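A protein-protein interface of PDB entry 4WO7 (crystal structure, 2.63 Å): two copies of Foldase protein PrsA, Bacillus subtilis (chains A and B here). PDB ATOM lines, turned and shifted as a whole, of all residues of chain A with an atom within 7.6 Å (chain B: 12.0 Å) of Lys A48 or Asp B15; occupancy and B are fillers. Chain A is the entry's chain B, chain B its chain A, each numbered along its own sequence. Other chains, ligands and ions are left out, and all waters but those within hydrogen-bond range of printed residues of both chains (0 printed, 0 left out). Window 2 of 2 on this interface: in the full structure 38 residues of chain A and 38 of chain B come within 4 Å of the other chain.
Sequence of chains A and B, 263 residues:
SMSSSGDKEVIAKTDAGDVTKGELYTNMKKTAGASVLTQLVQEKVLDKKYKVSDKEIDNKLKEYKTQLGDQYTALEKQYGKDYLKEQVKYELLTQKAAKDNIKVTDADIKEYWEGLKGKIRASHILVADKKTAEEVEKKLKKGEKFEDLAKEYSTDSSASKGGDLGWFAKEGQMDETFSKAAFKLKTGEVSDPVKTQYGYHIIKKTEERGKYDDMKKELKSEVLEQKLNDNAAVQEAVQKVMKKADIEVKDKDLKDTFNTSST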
ATOM      1  N   GLN A  42      30.704   1.895  19.142  1.00  0.00           N
ATOM      2  CA  GLN A  42      31.700   0.831  19.152  1.00  0.00           C
ATOM      3  C   GLN A  42      31.137  -0.497  19.658  1.00  0.00           C
ATOM      4  O   GLN A  42      31.488  -1.550  19.125  1.00  0.00           O
ATOM      5  CB  GLN A  42      32.918   1.228  19.995  1.00  0.00           C
ATOM      6  CG  GLN A  42      33.818   2.270  19.342  1.00  0.00           C
ATOM      7  CD  GLN A  42      35.026   2.620  20.198  1.00  0.00           C
ATOM      8  OE1 GLN A  42      35.243   2.031  21.259  1.00  0.00           O
ATOM      9  NE2 GLN A  42      35.826   3.573  19.735  1.00  0.00           N
ATOM     10  N   GLU A  43      30.270  -0.471  20.667  1.00  0.00           N
ATOM     11  CA  GLU A  43      29.748  -1.728  21.193  1.00  0.00           C
ATOM     12  C   GLU A  43      28.770  -2.352  20.198  1.00  0.00           C
ATOM     13  O   GLU A  43      28.568  -3.562  20.219  1.00  0.00           O
ATOM     14  CB  GLU A  43      29.097  -1.555  22.575  1.00  0.00           C
ATOM     15  CG  GLU A  43      27.678  -1.001  22.635  1.00  0.00           C
ATOM     16  CD  GLU A  43      27.251  -0.666  24.063  1.00  0.00           C
ATOM     17  OE1 GLU A  43      28.107  -0.701  24.975  1.00  0.00           O
ATOM     18  OE2 GLU A  43      26.053  -0.381  24.277  1.00  0.00           O
ATOM     19  N   LYS A  44      28.161  -1.541  19.334  1.00  0.00           N
ATOM     20  CA  LYS A  44      27.290  -2.083  18.289  1.00  0.00           C
ATOM     21  C   LYS A  44      28.117  -2.713  17.163  1.00  0.00           C
ATOM     22  O   LYS A  44      27.853  -3.836  16.726  1.00  0.00           O
ATOM     23  CB  LYS A  44      26.368  -1.005  17.711  1.00  0.00           C
ATOM     24  CG  LYS A  44      25.150  -0.738  18.568  1.00  0.00           C
ATOM     25  CD  LYS A  44      24.075   0.019  17.813  1.00  0.00           C
ATOM     26  CE  LYS A  44      22.803   0.134  18.642  1.00  0.00           C
ATOM     27  NZ  LYS A  44      22.930   1.033  19.824  1.00  0.00           N
ATOM     28  N   VAL A  45      29.112  -1.971  16.695  1.00  0.00           N
ATOM     29  CA  VAL A  45      29.944  -2.407  15.579  1.00  0.00           C
ATOM     30  C   VAL A  45      30.763  -3.641  15.946  1.00  0.00           C
ATOM     31  O   VAL A  45      30.801  -4.612  15.194  1.00  0.00           O
ATOM     32  CB  VAL A  45      30.881  -1.268  15.111  1.00  0.00           C
ATOM     33  CG1 VAL A  45      31.987  -1.784  14.173  1.00  0.00           C
ATOM     34  CG2 VAL A  45      30.075  -0.172  14.437  1.00  0.00           C
ATOM     35  N   LEU A  46      31.440  -3.593  17.089  1.00  0.00           N
ATOM     36  CA  LEU A  46      32.282  -4.708  17.512  1.00  0.00           C
ATOM     37  C   LEU A  46      31.465  -5.962  17.820  1.00  0.00           C
ATOM     38  O   LEU A  46      31.904  -7.075  17.533  1.00  0.00           O
ATOM     39  CB  LEU A  46      33.116  -4.318  18.737  1.00  0.00           C
ATOM     40  CG  LEU A  46      34.146  -3.202  18.529  1.00  0.00           C
ATOM     41  CD1 LEU A  46      34.896  -2.902  19.819  1.00  0.00           C
ATOM     42  CD2 LEU A  46      35.116  -3.556  17.412  1.00  0.00           C
ATOM     43  N   ASP A  47      30.283  -5.789  18.403  1.00  0.00           N
ATOM     44  CA  ASP A  47      29.446  -6.934  18.740  1.00  0.00           C
ATOM     45  C   ASP A  47      28.932  -7.590  17.461  1.00  0.00           C
ATOM     46  O   ASP A  47      28.542  -8.754  17.471  1.00  0.00           O
ATOM     47  CB  ASP A  47      28.281  -6.537  19.645  1.00  0.00           C
ATOM     48  CG  ASP A  47      27.511  -7.742  20.160  1.00  0.00           C
ATOM     49  OD1 ASP A  47      28.154  -8.770  20.476  1.00  0.00           O
ATOM     50  OD2 ASP A  47      26.268  -7.668  20.243  1.00  0.00           O
ATOM     51  N   LYS A  48      28.931  -6.838  16.362  1.00  0.00           N
ATOM     52  CA  LYS A  48      28.510  -7.375  15.071  1.00  0.00           C
ATOM     53  C   LYS A  48      29.615  -8.255  14.503  1.00  0.00           C
ATOM     54  O   LYS A  48      29.348  -9.292  13.897  1.00  0.00           O
ATOM     55  CB  LYS A  48      28.219  -6.247  14.079  1.00  0.00           C
ATOM     56  CG  LYS A  48      27.706  -6.697  12.718  1.00  0.00           C
ATOM     57  CD  LYS A  48      27.535  -5.494  11.812  1.00  0.00           C
ATOM     58  CE  LYS A  48      26.954  -5.863  10.467  1.00  0.00           C
ATOM     59  NZ  LYS A  48      26.826  -4.652   9.611  1.00  0.00           N
ATOM     60  N   LYS A  49      30.858  -7.827  14.709  1.00  0.00           N
ATOM     61  CA  LYS A  49      32.024  -8.568  14.243  1.00  0.00           C
ATOM     62  C   LYS A  49      32.403  -9.688  15.204  1.00  0.00           C
ATOM     63  O   LYS A  49      32.355 -10.867  14.851  1.00  0.00           O
ATOM     64  CB  LYS A  49      33.211  -7.619  14.043  1.00  0.00           C
ATOM     65  CG  LYS A  49      34.462  -8.297  13.498  1.00  0.00           C
ATOM     66  CD  LYS A  49      35.503  -7.295  13.018  1.00  0.00           C
ATOM     67  CE  LYS A  49      36.698  -8.017  12.417  1.00  0.00           C
ATOM     68  NZ  LYS A  49      37.745  -7.083  11.923  1.00  0.00           N
ATOM     69  N   TYR A  50      32.780  -9.306  16.420  1.00  0.00           N
ATOM     70  CA  TYR A  50      33.217 -10.262  17.431  1.00  0.00           C
ATOM     71  C   TYR A  50      32.066 -10.762  18.296  1.00  0.00           C
ATOM     72  O   TYR A  50      31.066 -10.072  18.484  1.00  0.00           O
ATOM     73  CB  TYR A  50      34.307  -9.631  18.303  1.00  0.00           C
ATOM     74  CG  TYR A  50      35.494  -9.162  17.496  1.00  0.00           C
ATOM     75  CD1 TYR A  50      36.509 -10.045  17.164  1.00  0.00           C
ATOM     76  CD2 TYR A  50      35.584  -7.857  17.037  1.00  0.00           C
ATOM     77  CE1 TYR A  50      37.594  -9.645  16.417  1.00  0.00           C
ATOM     78  CE2 TYR A  50      36.666  -7.443  16.281  1.00  0.00           C
ATOM     79  CZ  TYR A  50      37.666  -8.343  15.972  1.00  0.00           C
ATOM     80  OH  TYR A  50      38.743  -7.933  15.221  1.00  0.00           O
ATOM     81  N   LYS A  51      32.233 -11.974  18.815  1.00  0.00           N
ATOM     82  CA  LYS A  51      31.231 -12.612  19.658  1.00  0.00           C
ATOM     83  C   LYS A  51      31.888 -13.011  20.973  1.00  0.00           C
ATOM     84  O   LYS A  51      32.975 -13.590  20.980  1.00  0.00           O
ATOM     85  CB  LYS A  51      30.619 -13.816  18.937  1.00  0.00           C
ATOM     86  CG  LYS A  51      29.793 -13.398  17.725  1.00  0.00           C
ATOM     87  CD  LYS A  51      28.462 -12.772  18.119  1.00  0.00           C
ATOM     88  CE  LYS A  51      27.949 -11.824  17.039  1.00  0.00           C
ATOM     89  NZ  LYS A  51      27.665 -12.443  15.713  1.00  0.00           N
ATOM     90  N   LEU A  93      35.103  -6.974  24.076  1.00  0.00           N
ATOM     91  CA  LEU A  93      35.019  -6.669  22.655  1.00  0.00           C
ATOM     92  C   LEU A  93      36.185  -5.791  22.197  1.00  0.00           C
ATOM     93  O   LEU A  93      36.816  -6.089  21.184  1.00  0.00           O
ATOM     94  CB  LEU A  93      33.692  -5.988  22.313  1.00  0.00           C
ATOM     95  CG  LEU A  93      32.441  -6.874  22.314  1.00  0.00           C
ATOM     96  CD1 LEU A  93      31.185  -6.032  22.168  1.00  0.00           C
ATOM     97  CD2 LEU A  93      32.512  -7.929  21.221  1.00  0.00           C
ATOM     98  N   MET A 242      36.604   0.424  13.037  1.00  0.00           N
ATOM     99  CA  MET A 242      35.554   1.398  12.778  1.00  0.00           C
ATOM    100  C   MET A 242      35.664   1.967  11.370  1.00  0.00           C
ATOM    101  O   MET A 242      34.660   2.356  10.777  1.00  0.00           O
ATOM    102  CB  MET A 242      35.616   2.523  13.808  1.00  0.00           C
ATOM    103  CG  MET A 242      35.436   2.032  15.231  1.00  0.00           C
ATOM    104  SD  MET A 242      33.606   1.500  15.625  1.00  0.00           S
ATOM    105  CE  MET A 242      33.995  -0.255  16.397  1.00  0.00           C
ATOM    106  N   LYS A 244      36.203   0.446   8.638  1.00  0.00           N
ATOM    107  CA  LYS A 244      35.476  -0.419   7.714  1.00  0.00           C
ATOM    108  C   LYS A 244      33.945  -0.309   7.826  1.00  0.00           C
ATOM    109  O   LYS A 244      33.226  -0.830   6.971  1.00  0.00           O
ATOM    110  CB  LYS A 244      35.918  -1.878   7.914  1.00  0.00           C
ATOM    111  CG  LYS A 244      37.312  -2.234   7.340  1.00  0.00           C
ATOM    112  CD  LYS A 244      38.495  -1.529   8.018  1.00  0.00           C
ATOM    113  CE  LYS A 244      39.801  -1.777   7.253  1.00  0.00           C
ATOM    114  NZ  LYS A 244      40.981  -1.077   7.841  1.00  0.00           N
ATOM    115  N   ALA A 245      33.453   0.350   8.876  1.00  0.00           N
ATOM    116  CA  ALA A 245      32.013   0.579   9.066  1.00  0.00           C
ATOM    117  C   ALA A 245      31.608   2.001   8.673  1.00  0.00           C
ATOM    118  O   ALA A 245      32.441   2.908   8.650  1.00  0.00           O
ATOM    119  CB  ALA A 245      31.620   0.312  10.504  1.00  0.00           C
ATOM    120  N   ASP A 246      30.328   2.185   8.359  1.00  0.00           N
ATOM    121  CA  ASP A 246      29.808   3.491   7.966  1.00  0.00           C
ATOM    122  C   ASP A 246      29.096   4.202   9.119  1.00  0.00           C
ATOM    123  O   ASP A 246      27.911   3.967   9.357  1.00  0.00           O
ATOM    124  CB  ASP A 246      28.844   3.353   6.786  1.00  0.00           C
ATOM    125  CG  ASP A 246      28.158   4.661   6.444  1.00  0.00           C
ATOM    126  OD1 ASP A 246      28.874   5.651   6.181  1.00  0.00           O
ATOM    127  OD2 ASP A 246      26.909   4.703   6.456  1.00  0.00           O
ATOM    128  N   ILE A 247      29.812   5.073   9.825  1.00  0.00           N
ATOM    129  CA  ILE A 247      29.210   5.858  10.897  1.00  0.00           C
ATOM    130  C   ILE A 247      28.778   7.206  10.337  1.00  0.00           C
ATOM    131  O   ILE A 247      29.583   7.904   9.720  1.00  0.00           O
ATOM    132  CB  ILE A 247      30.187   6.119  12.062  1.00  0.00           C
ATOM    133  CG1 ILE A 247      31.104   4.915  12.314  1.00  0.00           C
ATOM    134  CG2 ILE A 247      29.422   6.527  13.316  1.00  0.00           C
ATOM    135  CD1 ILE A 247      30.392   3.604  12.604  1.00  0.00           C
ATOM    136  N   GLU A 248      27.507   7.551  10.528  1.00  0.00           N
ATOM    137  CA  GLU A 248      26.986   8.847  10.108  1.00  0.00           C
ATOM    138  C   GLU A 248      26.230   9.483  11.270  1.00  0.00           C
ATOM    139  O   GLU A 248      25.096   9.110  11.576  1.00  0.00           O
ATOM    140  CB  GLU A 248      26.081   8.690   8.882  1.00  0.00           C
ATOM    141  CG  GLU A 248      25.565   9.985   8.281  1.00  0.00           C
ATOM    142  CD  GLU A 248      24.746   9.736   7.026  1.00  0.00           C
ATOM    143  OE1 GLU A 248      24.603   8.557   6.634  1.00  0.00           O
ATOM    144  OE2 GLU A 248      24.241  10.713   6.435  1.00  0.00           O
ATOM    145  N   VAL B  10      17.128   9.613  15.787  1.00  0.00           N
ATOM    146  CA  VAL B  10      18.389   8.945  15.497  1.00  0.00           C
ATOM    147  C   VAL B  10      19.539   9.922  15.672  1.00  0.00           C
ATOM    148  O   VAL B  10      19.634  10.921  14.961  1.00  0.00           O
ATOM    149  CB  VAL B  10      18.407   8.354  14.073  1.00  0.00           C
ATOM    150  CG1 VAL B  10      19.794   7.809  13.716  1.00  0.00           C
ATOM    151  CG2 VAL B  10      17.364   7.257  13.948  1.00  0.00           C
ATOM    152  N   ILE B  11      20.418   9.612  16.620  1.00  0.00           N
ATOM    153  CA  ILE B  11      21.591  10.433  16.879  1.00  0.00           C
ATOM    154  C   ILE B  11      22.671  10.119  15.862  1.00  0.00           C
ATOM    155  O   ILE B  11      23.289  11.020  15.288  1.00  0.00           O
ATOM    156  CB  ILE B  11      22.160  10.177  18.287  1.00  0.00           C
ATOM    157  CG1 ILE B  11      21.118  10.479  19.368  1.00  0.00           C
ATOM    158  CG2 ILE B  11      23.455  10.970  18.500  1.00  0.00           C
ATOM    159  CD1 ILE B  11      20.684  11.920  19.426  1.00  0.00           C
ATOM    160  N   ALA B  12      22.886   8.826  15.647  1.00  0.00           N
ATOM    161  CA  ALA B  12      23.907   8.356  14.724  1.00  0.00           C
ATOM    162  C   ALA B  12      23.409   7.143  13.960  1.00  0.00           C
ATOM    163  O   ALA B  12      22.835   6.219  14.539  1.00  0.00           O
ATOM    164  CB  ALA B  12      25.189   8.019  15.478  1.00  0.00           C
ATOM    165  N   LYS B  13      23.648   7.149  12.655  1.00  0.00           N
ATOM    166  CA  LYS B  13      23.265   6.042  11.798  1.00  0.00           C
ATOM    167  C   LYS B  13      24.481   5.196  11.478  1.00  0.00           C
ATOM    168  O   LYS B  13      25.534   5.714  11.098  1.00  0.00           O
ATOM    169  CB  LYS B  13      22.610   6.555  10.512  1.00  0.00           C
ATOM    170  CG  LYS B  13      21.874   5.477   9.731  1.00  0.00           C
ATOM    171  CD  LYS B  13      21.279   6.013   8.436  1.00  0.00           C
ATOM    172  CE  LYS B  13      20.806   4.883   7.531  1.00  0.00           C
ATOM    173  NZ  LYS B  13      19.668   4.126   8.106  1.00  0.00           N
ATOM    174  N   THR B  14      24.316   3.886  11.623  1.00  0.00           N
ATOM    175  CA  THR B  14      25.390   2.931  11.388  1.00  0.00           C
ATOM    176  C   THR B  14      24.838   1.672  10.715  1.00  0.00           C
ATOM    177  O   THR B  14      23.674   1.317  10.906  1.00  0.00           O
ATOM    178  CB  THR B  14      26.096   2.588  12.725  1.00  0.00           C
ATOM    179  OG1 THR B  14      26.534   3.802  13.356  1.00  0.00           O
ATOM    180  CG2 THR B  14      27.293   1.672  12.530  1.00  0.00           C
ATOM    181  N   ASP B  15      25.669   1.014   9.911  1.00  0.00           N
ATOM    182  CA  ASP B  15      25.279  -0.226   9.235  1.00  0.00           C
ATOM    183  C   ASP B  15      25.128  -1.396  10.220  1.00  0.00           C
ATOM    184  O   ASP B  15      24.463  -2.387   9.923  1.00  0.00           O
ATOM    185  CB  ASP B  15      26.284  -0.553   8.124  1.00  0.00           C
ATOM    186  CG  ASP B  15      27.720  -0.516   8.602  1.00  0.00           C
ATOM    187  OD1 ASP B  15      27.965  -0.011   9.718  1.00  0.00           O
ATOM    188  OD2 ASP B  15      28.605  -0.974   7.850  1.00  0.00           O
ATOM    189  N   ALA B  16      25.758  -1.267  11.384  1.00  0.00           N
ATOM    190  CA  ALA B  16      25.623  -2.223  12.486  1.00  0.00           C
ATOM    191  C   ALA B  16      24.514  -1.817  13.474  1.00  0.00           C
ATOM    192  O   ALA B  16      24.439  -2.352  14.581  1.00  0.00           O
ATOM    193  CB  ALA B  16      26.953  -2.352  13.228  1.00  0.00           C
ATOM    194  N   GLY B  17      23.667  -0.869  13.070  1.00  0.00           N
ATOM    195  CA  GLY B  17      22.503  -0.459  13.851  1.00  0.00           C
ATOM    196  C   GLY B  17      22.571   0.989  14.304  1.00  0.00           C
ATOM    197  O   GLY B  17      23.658   1.514  14.488  1.00  0.00           O
ATOM    198  N   ASP B  18      21.422   1.621  14.542  1.00  0.00           N
ATOM    199  CA  ASP B  18      21.402   3.038  14.925  1.00  0.00           C
ATOM    200  C   ASP B  18      21.446   3.267  16.422  1.00  0.00           C
ATOM    201  O   ASP B  18      21.027   2.427  17.214  1.00  0.00           O
ATOM    202  CB  ASP B  18      20.160   3.731  14.356  1.00  0.00           C
ATOM    203  CG  ASP B  18      20.067   3.607  12.856  1.00  0.00           C
ATOM    204  OD1 ASP B  18      21.119   3.368  12.226  1.00  0.00           O
ATOM    205  OD2 ASP B  18      18.955   3.747  12.308  1.00  0.00           O
ATOM    206  N   VAL B  19      21.940   4.445  16.782  1.00  0.00           N
ATOM    207  CA  VAL B  19      21.924   4.931  18.149  1.00  0.00           C
ATOM    208  C   VAL B  19      20.845   5.997  18.282  1.00  0.00           C
ATOM    209  O   VAL B  19      20.890   7.021  17.600  1.00  0.00           O
ATOM    210  CB  VAL B  19      23.307   5.490  18.529  1.00  0.00           C
ATOM    211  CG1 VAL B  19      23.287   6.121  19.909  1.00  0.00           C
ATOM    212  CG2 VAL B  19      24.361   4.382  18.445  1.00  0.00           C
ATOM    213  N   THR B  20      19.871   5.747  19.152  1.00  0.00           N
ATOM    214  CA  THR B  20      18.762   6.673  19.346  1.00  0.00           C
ATOM    215  C   THR B  20      19.030   7.663  20.484  1.00  0.00           C
ATOM    216  O   THR B  20      19.928   7.460  21.301  1.00  0.00           O
ATOM    217  CB  THR B  20      17.464   5.912  19.642  1.00  0.00           C
ATOM    218  OG1 THR B  20      17.627   5.124  20.827  1.00  0.00           O
ATOM    219  CG2 THR B  20      17.087   5.010  18.465  1.00  0.00           C
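N of Lys B13 is in hydrogen-bond range of O of Glu A248 (2.7 Å). The backbone carbonyl oxygen (O) of Asp B15 sits at hydrogen-bond distance from the side-chain amino group (NZ) of Lys A48. The backbone carbonyl oxygen of Asp A246 lies close to the backbone carbonyl oxygen of Lys B13 (3.4 Å).
The backbone NH (N) of Ile B11 sits at hydrogen-bond distance from the backbone carbonyl oxygen (O) of Val B19, at 2.8 Å. The backbone carbonyl oxygen (O) of Ala B12 lies within hydrogen-bond range of the backbone NH (N) of Val B19, at 3.0 Å. The backbone NH (N) of Thr B14 is in hydrogen-bond range of the side-chain carboxylate (OD1) of Asp B18 (3.3 Å).
Among the printed residues, pairs that only touch across the chains: Lys A44 with Ala B16 (3.9 Å), Lys A44 with Gly B17 (3.7 Å), Lys A44 with Asp B18 (3.2 Å), Lys A44 with Val B19 (3.9 Å), Val A45 with Thr B14 (3.8 Å), Val A45 with Ala B16 (3.8 Å), Lys A48 with Ala B16 (3.5 Å), Ala A245 with Asp B15 (3.8 Å), Asp A246 with Thr B14 (3.4 Å), Asp A246 with Asp B15 (3.5 Å), Ile A247 with Lys B13 (3.7 Å), Ile A247 with Thr B14 (3.7 Å) and Glu A248 with Ala B12 (3.4 Å).
Printed residues of chain B within 4 Å of Lys A44: Ala B16, Gly B17, Asp B18 and Val B19. Val A45 touches just these residues of chain B: Thr B14 (3.8 Å) and Ala B16 (3.8 Å). No residue of chain B comes within 4 Å of Asp A47. Lys A48 touches two residues of chain B. Asp A246 touches three residues of chain B. Of chain B, only Lys B13 (3.7 Å) and Thr B14 (3.7 Å) come within 4 Å of Ile A247. Printed residues of chain B within 4 Å of Glu A248: Ala B12 (3.4 Å) and Lys B13 (2.7 Å). Of the printed residues of chain A, Lys B13 touches Asp A246 (3.4 Å), Ile A247 (3.7 Å) and Glu A248 (2.7 Å). Asp B15 touches three residues of chain A. Printed residues of chain A within 4 Å of Asp B18: Lys A44 (3.2 Å). Of the printed residues of chain A, Val B19 touches Lys A44 (3.9 Å). The nearest residue of chain A that does not touch Asp B15 is Lys A244 (4.7 Å). The nearest printed residue of chain A that does not touch Gly B17 is Lys A48 (6.0 Å).
Of the 11 printed residues of chain B, 8 touch a printed residue of chain A. Hydrophobic or aromatic side chains of chain A within 4 Å of the printed part of chain B: Val A45, Ala A245 and Ile A247.
No position is printed for both chains. Of the 16 pairs that touch across the chains among the printed residues, none has its exchanged pair printed and touching as well.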
